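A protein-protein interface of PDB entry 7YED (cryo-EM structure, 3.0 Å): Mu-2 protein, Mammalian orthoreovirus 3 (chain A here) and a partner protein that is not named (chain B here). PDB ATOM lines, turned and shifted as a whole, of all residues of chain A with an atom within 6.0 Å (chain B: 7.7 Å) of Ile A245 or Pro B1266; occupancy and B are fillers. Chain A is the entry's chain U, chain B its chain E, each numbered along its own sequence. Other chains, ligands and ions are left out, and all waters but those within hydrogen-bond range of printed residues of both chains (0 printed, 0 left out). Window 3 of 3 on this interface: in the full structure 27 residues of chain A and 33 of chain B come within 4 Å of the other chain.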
ATOM      1  N   TYR A  65      38.119 -12.904  24.391  1.00  0.00           N
ATOM      2  CA  TYR A  65      38.417 -12.606  22.987  1.00  0.00           C
ATOM      3  C   TYR A  65      39.865 -12.176  22.779  1.00  0.00           C
ATOM      4  O   TYR A  65      40.129 -11.168  22.131  1.00  0.00           O
ATOM      5  CB  TYR A  65      37.470 -11.531  22.466  1.00  0.00           C
ATOM      6  CG  TYR A  65      36.026 -11.947  22.345  1.00  0.00           C
ATOM      7  CD1 TYR A  65      35.654 -13.269  22.434  1.00  0.00           C
ATOM      8  CD2 TYR A  65      35.036 -11.008  22.122  1.00  0.00           C
ATOM      9  CE1 TYR A  65      34.337 -13.641  22.323  1.00  0.00           C
ATOM     10  CE2 TYR A  65      33.719 -11.368  22.014  1.00  0.00           C
ATOM     11  CZ  TYR A  65      33.372 -12.688  22.110  1.00  0.00           C
ATOM     12  OH  TYR A  65      32.055 -13.062  21.997  1.00  0.00           O
ATOM     13  N   ILE A 210      38.432 -17.683  21.921  1.00  0.00           N
ATOM     14  CA  ILE A 210      37.754 -18.050  20.686  1.00  0.00           C
ATOM     15  C   ILE A 210      38.170 -17.079  19.591  1.00  0.00           C
ATOM     16  O   ILE A 210      37.386 -16.761  18.694  1.00  0.00           O
ATOM     17  CB  ILE A 210      36.227 -18.089  20.867  1.00  0.00           C
ATOM     18  CG1 ILE A 210      35.675 -16.715  21.213  1.00  0.00           C
ATOM     19  CG2 ILE A 210      35.856 -19.060  21.960  1.00  0.00           C
ATOM     20  CD1 ILE A 210      34.171 -16.695  21.205  1.00  0.00           C
ATOM     21  N   ILE A 241      28.294 -19.644  28.476  1.00  0.00           N
ATOM     22  CA  ILE A 241      27.854 -18.673  27.479  1.00  0.00           C
ATOM     23  C   ILE A 241      28.321 -19.059  26.084  1.00  0.00           C
ATOM     24  O   ILE A 241      27.662 -18.739  25.091  1.00  0.00           O
ATOM     25  CB  ILE A 241      28.355 -17.264  27.832  1.00  0.00           C
ATOM     26  CG1 ILE A 241      27.745 -16.797  29.147  1.00  0.00           C
ATOM     27  CG2 ILE A 241      28.019 -16.290  26.730  1.00  0.00           C
ATOM     28  CD1 ILE A 241      28.364 -15.534  29.663  1.00  0.00           C
ATOM     29  N   HIS A 242      29.443 -19.762  25.993  1.00  0.00           N
ATOM     30  CA  HIS A 242      30.032 -20.123  24.710  1.00  0.00           C
ATOM     31  C   HIS A 242      30.111 -21.632  24.564  1.00  0.00           C
ATOM     32  O   HIS A 242      31.069 -22.171  24.011  1.00  0.00           O
ATOM     33  CB  HIS A 242      31.416 -19.504  24.551  1.00  0.00           C
ATOM     34  CG  HIS A 242      31.413 -18.009  24.510  1.00  0.00           C
ATOM     35  ND1 HIS A 242      31.000 -17.297  23.405  1.00  0.00           N
ATOM     36  CD2 HIS A 242      31.784 -17.090  25.431  1.00  0.00           C
ATOM     37  CE1 HIS A 242      31.111 -16.005  23.651  1.00  0.00           C
ATOM     38  NE2 HIS A 242      31.584 -15.852  24.874  1.00  0.00           N
ATOM     39  N   ALA A 243      29.096 -22.334  25.063  1.00  0.00           N
ATOM     40  CA  ALA A 243      29.148 -23.791  25.085  1.00  0.00           C
ATOM     41  C   ALA A 243      29.150 -24.370  23.679  1.00  0.00           C
ATOM     42  O   ALA A 243      29.886 -25.320  23.394  1.00  0.00           O
ATOM     43  CB  ALA A 243      27.973 -24.340  25.889  1.00  0.00           C
ATOM     44  N   ASN A 244      28.344 -23.807  22.785  1.00  0.00           N
ATOM     45  CA  ASN A 244      28.118 -24.408  21.479  1.00  0.00           C
ATOM     46  C   ASN A 244      29.215 -24.102  20.469  1.00  0.00           C
ATOM     47  O   ASN A 244      29.236 -24.726  19.404  1.00  0.00           O
ATOM     48  CB  ASN A 244      26.773 -23.939  20.928  1.00  0.00           C
ATOM     49  CG  ASN A 244      25.607 -24.482  21.714  1.00  0.00           C
ATOM     50  OD1 ASN A 244      25.579 -25.657  22.069  1.00  0.00           O
ATOM     51  ND2 ASN A 244      24.640 -23.625  22.004  1.00  0.00           N
ATOM     52  N   ILE A 245      30.126 -23.175  20.764  1.00  0.00           N
ATOM     53  CA  ILE A 245      31.130 -22.747  19.800  1.00  0.00           C
ATOM     54  C   ILE A 245      32.550 -23.054  20.245  1.00  0.00           C
ATOM     55  O   ILE A 245      33.493 -22.692  19.539  1.00  0.00           O
ATOM     56  CB  ILE A 245      30.994 -21.247  19.476  1.00  0.00           C
ATOM     57  CG1 ILE A 245      31.230 -20.412  20.729  1.00  0.00           C
ATOM     58  CG2 ILE A 245      29.628 -20.957  18.896  1.00  0.00           C
ATOM     59  CD1 ILE A 245      31.343 -18.938  20.455  1.00  0.00           C
ATOM     60  N   LEU A 246      32.737 -23.700  21.390  1.00  0.00           N
ATOM     61  CA  LEU A 246      34.069 -24.077  21.834  1.00  0.00           C
ATOM     62  C   LEU A 246      34.449 -25.432  21.257  1.00  0.00           C
ATOM     63  O   LEU A 246      33.591 -26.271  20.976  1.00  0.00           O
ATOM     64  CB  LEU A 246      34.148 -24.121  23.359  1.00  0.00           C
ATOM     65  CG  LEU A 246      34.002 -22.797  24.105  1.00  0.00           C
ATOM     66  CD1 LEU A 246      33.966 -23.040  25.598  1.00  0.00           C
ATOM     67  CD2 LEU A 246      35.136 -21.863  23.750  1.00  0.00           C
ATOM     68  N   ASN A 247      35.750 -25.642  21.084  1.00  0.00           N
ATOM     69  CA  ASN A 247      36.278 -26.886  20.535  1.00  0.00           C
ATOM     70  C   ASN A 247      36.807 -27.742  21.677  1.00  0.00           C
ATOM     71  O   ASN A 247      37.876 -27.462  22.229  1.00  0.00           O
ATOM     72  CB  ASN A 247      37.372 -26.606  19.508  1.00  0.00           C
ATOM     73  CG  ASN A 247      36.859 -25.861  18.297  1.00  0.00           C
ATOM     74  OD1 ASN A 247      37.257 -24.726  18.038  1.00  0.00           O
ATOM     75  ND2 ASN A 247      35.968 -26.495  17.546  1.00  0.00           N
ATOM     76  N   ARG B 254      23.485 -27.039  25.386  1.00  0.00           N
ATOM     77  CA  ARG B 254      24.464 -27.607  24.466  1.00  0.00           C
ATOM     78  C   ARG B 254      23.699 -28.266  23.326  1.00  0.00           C
ATOM     79  O   ARG B 254      23.164 -29.365  23.478  1.00  0.00           O
ATOM     80  CB  ARG B 254      25.370 -28.597  25.187  1.00  0.00           C
ATOM     81  CG  ARG B 254      26.437 -29.213  24.313  1.00  0.00           C
ATOM     82  CD  ARG B 254      27.458 -28.178  23.895  1.00  0.00           C
ATOM     83  NE  ARG B 254      28.485 -28.735  23.024  1.00  0.00           N
ATOM     84  CZ  ARG B 254      29.631 -29.252  23.452  1.00  0.00           C
ATOM     85  NH1 ARG B 254      29.900 -29.282  24.747  1.00  0.00           N
ATOM     86  NH2 ARG B 254      30.506 -29.737  22.582  1.00  0.00           N
ATOM     87  N   VAL B 256      24.879 -28.248  19.641  1.00  0.00           N
ATOM     88  CA  VAL B 256      25.690 -28.791  18.558  1.00  0.00           C
ATOM     89  C   VAL B 256      26.744 -29.716  19.155  1.00  0.00           C
ATOM     90  O   VAL B 256      27.661 -29.265  19.843  1.00  0.00           O
ATOM     91  CB  VAL B 256      26.336 -27.675  17.732  1.00  0.00           C
ATOM     92  CG1 VAL B 256      27.242 -28.267  16.674  1.00  0.00           C
ATOM     93  CG2 VAL B 256      25.268 -26.808  17.100  1.00  0.00           C
ATOM     94  N   ARG B 503      28.738 -22.427   6.910  1.00  0.00           N
ATOM     95  CA  ARG B 503      28.666 -22.369   8.360  1.00  0.00           C
ATOM     96  C   ARG B 503      27.310 -22.855   8.862  1.00  0.00           C
ATOM     97  O   ARG B 503      26.345 -22.979   8.108  1.00  0.00           O
ATOM     98  CB  ARG B 503      28.911 -20.943   8.840  1.00  0.00           C
ATOM     99  CG  ARG B 503      30.306 -20.469   8.551  1.00  0.00           C
ATOM    100  CD  ARG B 503      30.519 -19.050   8.996  1.00  0.00           C
ATOM    101  NE  ARG B 503      31.891 -18.639   8.734  1.00  0.00           N
ATOM    102  CZ  ARG B 503      32.289 -18.075   7.603  1.00  0.00           C
ATOM    103  NH1 ARG B 503      31.416 -17.853   6.635  1.00  0.00           N
ATOM    104  NH2 ARG B 503      33.560 -17.733   7.442  1.00  0.00           N
ATOM    105  N   LEU B 504      27.249 -23.129  10.164  1.00  0.00           N
ATOM    106  CA  LEU B 504      26.017 -23.516  10.840  1.00  0.00           C
ATOM    107  C   LEU B 504      25.927 -22.759  12.153  1.00  0.00           C
ATOM    108  O   LEU B 504      26.794 -22.909  13.015  1.00  0.00           O
ATOM    109  CB  LEU B 504      25.966 -25.022  11.099  1.00  0.00           C
ATOM    110  CG  LEU B 504      24.701 -25.509  11.804  1.00  0.00           C
ATOM    111  CD1 LEU B 504      23.481 -25.240  10.953  1.00  0.00           C
ATOM    112  CD2 LEU B 504      24.803 -26.981  12.121  1.00  0.00           C
ATOM    113  N   MET B 505      24.880 -21.953  12.310  1.00  0.00           N
ATOM    114  CA  MET B 505      24.672 -21.187  13.536  1.00  0.00           C
ATOM    115  C   MET B 505      23.186 -21.157  13.858  1.00  0.00           C
ATOM    116  O   MET B 505      22.440 -20.293  13.382  1.00  0.00           O
ATOM    117  CB  MET B 505      25.275 -19.786  13.421  1.00  0.00           C
ATOM    118  CG  MET B 505      24.770 -18.949  12.265  1.00  0.00           C
ATOM    119  SD  MET B 505      25.627 -17.367  12.129  1.00  0.00           S
ATOM    120  CE  MET B 505      27.197 -17.887  11.458  1.00  0.00           C
ATOM    121  N   PRO B 506      22.722 -22.093  14.671  1.00  0.00           N
ATOM    122  CA  PRO B 506      21.285 -22.232  14.924  1.00  0.00           C
ATOM    123  C   PRO B 506      20.740 -21.229  15.925  1.00  0.00           C
ATOM    124  O   PRO B 506      20.687 -21.522  17.121  1.00  0.00           O
ATOM    125  CB  PRO B 506      21.175 -23.660  15.465  1.00  0.00           C
ATOM    126  CG  PRO B 506      22.480 -23.895  16.117  1.00  0.00           C
ATOM    127  CD  PRO B 506      23.500 -23.171  15.298  1.00  0.00           C
ATOM    128  N   TYR B 507      20.334 -20.049  15.465  1.00  0.00           N
ATOM    129  CA  TYR B 507      19.846 -19.016  16.367  1.00  0.00           C
ATOM    130  C   TYR B 507      18.403 -18.587  16.136  1.00  0.00           C
ATOM    131  O   TYR B 507      17.724 -18.253  17.106  1.00  0.00           O
ATOM    132  CB  TYR B 507      20.751 -17.784  16.285  1.00  0.00           C
ATOM    133  CG  TYR B 507      22.132 -18.057  16.816  1.00  0.00           C
ATOM    134  CD1 TYR B 507      22.361 -18.119  18.175  1.00  0.00           C
ATOM    135  CD2 TYR B 507      23.200 -18.265  15.963  1.00  0.00           C
ATOM    136  CE1 TYR B 507      23.612 -18.369  18.675  1.00  0.00           C
ATOM    137  CE2 TYR B 507      24.460 -18.519  16.455  1.00  0.00           C
ATOM    138  CZ  TYR B 507      24.658 -18.571  17.812  1.00  0.00           C
ATOM    139  OH  TYR B 507      25.911 -18.825  18.314  1.00  0.00           O
ATOM    140  N   THR B 912      27.183 -11.244  22.497  1.00  0.00           N
ATOM    141  CA  THR B 912      26.223 -12.085  21.792  1.00  0.00           C
ATOM    142  C   THR B 912      25.389 -12.916  22.760  1.00  0.00           C
ATOM    143  O   THR B 912      24.954 -14.018  22.423  1.00  0.00           O
ATOM    144  CB  THR B 912      26.939 -12.992  20.795  1.00  0.00           C
ATOM    145  OG1 THR B 912      27.821 -13.871  21.503  1.00  0.00           O
ATOM    146  CG2 THR B 912      27.760 -12.163  19.822  1.00  0.00           C
ATOM    147  N   GLN B 919      18.540 -19.630  22.088  1.00  0.00           N
ATOM    148  CA  GLN B 919      18.696 -21.082  22.128  1.00  0.00           C
ATOM    149  C   GLN B 919      18.063 -21.676  23.385  1.00  0.00           C
ATOM    150  O   GLN B 919      17.418 -22.738  23.337  1.00  0.00           O
ATOM    151  CB  GLN B 919      20.171 -21.455  22.035  1.00  0.00           C
ATOM    152  CG  GLN B 919      20.789 -21.132  20.696  1.00  0.00           C
ATOM    153  CD  GLN B 919      22.247 -21.495  20.635  1.00  0.00           C
ATOM    154  OE1 GLN B 919      22.831 -21.921  21.626  1.00  0.00           O
ATOM    155  NE2 GLN B 919      22.849 -21.338  19.467  1.00  0.00           N
ATOM    156  N   GLU B1263      30.970 -25.962   9.958  1.00  0.00           N
ATOM    157  CA  GLU B1263      31.735 -25.336  11.019  1.00  0.00           C
ATOM    158  C   GLU B1263      30.869 -24.301  11.716  1.00  0.00           C
ATOM    159  O   GLU B1263      30.021 -23.657  11.095  1.00  0.00           O
ATOM    160  CB  GLU B1263      33.003 -24.684  10.481  1.00  0.00           C
ATOM    161  CG  GLU B1263      32.753 -23.482   9.609  1.00  0.00           C
ATOM    162  CD  GLU B1263      34.033 -22.903   9.053  1.00  0.00           C
ATOM    163  OE1 GLU B1263      35.105 -23.500   9.284  1.00  0.00           O
ATOM    164  OE2 GLU B1263      33.972 -21.840   8.403  1.00  0.00           O
ATOM    165  N   THR B1264      31.087 -24.146  13.021  1.00  0.00           N
ATOM    166  CA  THR B1264      30.252 -23.307  13.877  1.00  0.00           C
ATOM    167  C   THR B1264      31.119 -22.223  14.505  1.00  0.00           C
ATOM    168  O   THR B1264      31.544 -22.347  15.661  1.00  0.00           O
ATOM    169  CB  THR B1264      29.566 -24.139  14.953  1.00  0.00           C
ATOM    170  OG1 THR B1264      30.561 -24.756  15.779  1.00  0.00           O
ATOM    171  CG2 THR B1264      28.720 -25.218  14.319  1.00  0.00           C
ATOM    172  N   PRO B1265      31.396 -21.149  13.778  1.00  0.00           N
ATOM    173  CA  PRO B1265      32.216 -20.077  14.325  1.00  0.00           C
ATOM    174  C   PRO B1265      31.380 -19.150  15.185  1.00  0.00           C
ATOM    175  O   PRO B1265      30.152 -19.089  15.030  1.00  0.00           O
ATOM    176  CB  PRO B1265      32.721 -19.355  13.073  1.00  0.00           C
ATOM    177  CG  PRO B1265      31.634 -19.565  12.094  1.00  0.00           C
ATOM    178  CD  PRO B1265      31.080 -20.928  12.359  1.00  0.00           C
ATOM    179  N   PRO B1266      32.002 -18.414  16.098  1.00  0.00           N
ATOM    180  CA  PRO B1266      31.262 -17.397  16.844  1.00  0.00           C
ATOM    181  C   PRO B1266      30.835 -16.268  15.923  1.00  0.00           C
ATOM    182  O   PRO B1266      31.464 -16.003  14.898  1.00  0.00           O
ATOM    183  CB  PRO B1266      32.271 -16.918  17.888  1.00  0.00           C
ATOM    184  CG  PRO B1266      33.591 -17.196  17.274  1.00  0.00           C
ATOM    185  CD  PRO B1266      33.425 -18.448  16.472  1.00  0.00           C
ATOM    186  N   ILE B1267      29.741 -15.602  16.301  1.00  0.00           N
ATOM    187  CA  ILE B1267      29.186 -14.544  15.461  1.00  0.00           C
ATOM    188  C   ILE B1267      30.174 -13.404  15.281  1.00  0.00           C
ATOM    189  O   ILE B1267      30.200 -12.755  14.228  1.00  0.00           O
ATOM    190  CB  ILE B1267      27.861 -14.037  16.055  1.00  0.00           C
ATOM    191  CG1 ILE B1267      26.816 -15.148  16.050  1.00  0.00           C
ATOM    192  CG2 ILE B1267      27.364 -12.839  15.283  1.00  0.00           C
ATOM    193  CD1 ILE B1267      25.582 -14.812  16.840  1.00  0.00           C
ATOM    194  N   THR B1268      30.993 -13.133  16.295  1.00  0.00           N
ATOM    195  CA  THR B1268      31.909 -12.003  16.220  1.00  0.00           C
ATOM    196  C   THR B1268      33.065 -12.254  15.267  1.00  0.00           C
ATOM    197  O   THR B1268      33.710 -11.295  14.833  1.00  0.00           O
ATOM    198  CB  THR B1268      32.451 -11.672  17.606  1.00  0.00           C
ATOM    199  OG1 THR B1268      33.169 -12.799  18.116  1.00  0.00           O
ATOM    200  CG2 THR B1268      31.315 -11.338  18.546  1.00  0.00           C
ATOM    201  N   ALA B1269      33.350 -13.510  14.939  1.00  0.00           N
ATOM    202  CA  ALA B1269      34.402 -13.808  13.982  1.00  0.00           C
ATOM    203  C   ALA B1269      33.943 -13.658  12.542  1.00  0.00           C
ATOM    204  O   ALA B1269      34.781 -13.670  11.635  1.00  0.00           O
ATOM    205  CB  ALA B1269      34.932 -15.222  14.204  1.00  0.00           C
ATOM    206  N   VAL B1270      32.642 -13.516  12.311  1.00  0.00           N
ATOM    207  CA  VAL B1270      32.091 -13.420  10.972  1.00  0.00           C
ATOM    208  C   VAL B1270      31.498 -12.045  10.701  1.00  0.00           C
ATOM    209  O   VAL B1270      31.607 -11.532   9.587  1.00  0.00           O
ATOM    210  CB  VAL B1270      31.042 -14.525  10.736  1.00  0.00           C
ATOM    211  CG1 VAL B1270      30.413 -14.352   9.382  1.00  0.00           C
ATOM    212  CG2 VAL B1270      31.685 -15.886  10.851  1.00  0.00           C
ATOM    213  N   VAL B1271      30.864 -11.439  11.695  1.00  0.00           N
ATOM    214  CA  VAL B1271      30.268 -10.117  11.558  1.00  0.00           C
ATOM    215  C   VAL B1271      31.125  -9.155  12.371  1.00  0.00           C
ATOM    216  O   VAL B1271      30.980  -9.059  13.593  1.00  0.00           O
ATOM    217  CB  VAL B1271      28.807 -10.097  12.016  1.00  0.00           C
ATOM    218  CG1 VAL B1271      28.261  -8.691  11.974  1.00  0.00           C
ATOM    219  CG2 VAL B1271      27.976 -11.010  11.147  1.00  0.00           C
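Tyr A65 touches Thr B1268 (OH to CG2, 3.9 Å).
CD1 of Ile A210 touches CB of Pro B1266 (3.8 Å).
Ala A243 touches Arg B254 (O to NE, 3.7 Å).
Asn A244 touches Arg B254.
Asn A244 touches Val B256 (OD1 to N, 3.6 Å).
O of Asn A244 touches OG1 of Thr B1264 (3.9 Å).
CD1 of Ile A245 touches CB of Pro B1266, 3.4 Å away.
The backbone carbonyl oxygen of Val B256 lies within hydrogen-bond range of the guanidinium group of Arg B254 (3.3 Å).
The side-chain amide nitrogen of Gln B919 sits at hydrogen-bond distance from the backbone carbonyl oxygen of Pro B506 (3.2 Å).
Printed residues of chain B within 4 Å of Ile A245: Pro B1266.
Pro B1266 touches just these residues of chain A: Ile A210 and Ile A245.
Of the printed residues of chain B, Tyr A65 touches Thr B1268.
Of the printed residues of chain A, Thr B1264 touches Asn A244 (3.9 Å).
Printed residues of chain B within 4 Å of Ala A243: Arg B254.
Of the printed residues of chain A, Arg B254 touches Ala A243 (3.7 Å) and Asn A244 (3.3 Å).
Ile A241 touches none of the printed residues of chain B.
The nearest residue of chain A that does not touch Pro B1266 is Tyr A65 (5.6 Å).
The nearest printed residue of chain B that does not touch Tyr A65 is Thr B912 (4.3 Å).
The side-chain amide oxygen of Gln B919 sits at hydrogen-bond distance from the side-chain amide nitrogen of Asn A244 (2.5 Å).
Of the 18 printed residues of chain B, 6 touch a printed residue of chain A.
Printed residues of chain B that touch a printed residue of chain A: Arg B254, Val B256, Gln B919, Thr B1264, Pro B1266 and Thr B1268.
Of the 9 printed residues of chain A, 5 touch a printed residue of chain B.
Among the printed residues, 8 pairs touch across the chains.
Among the printed residues, no Asp or Glu carboxylate lies within 4 Å of a Lys or Arg side-chain nitrogen of the other chain.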
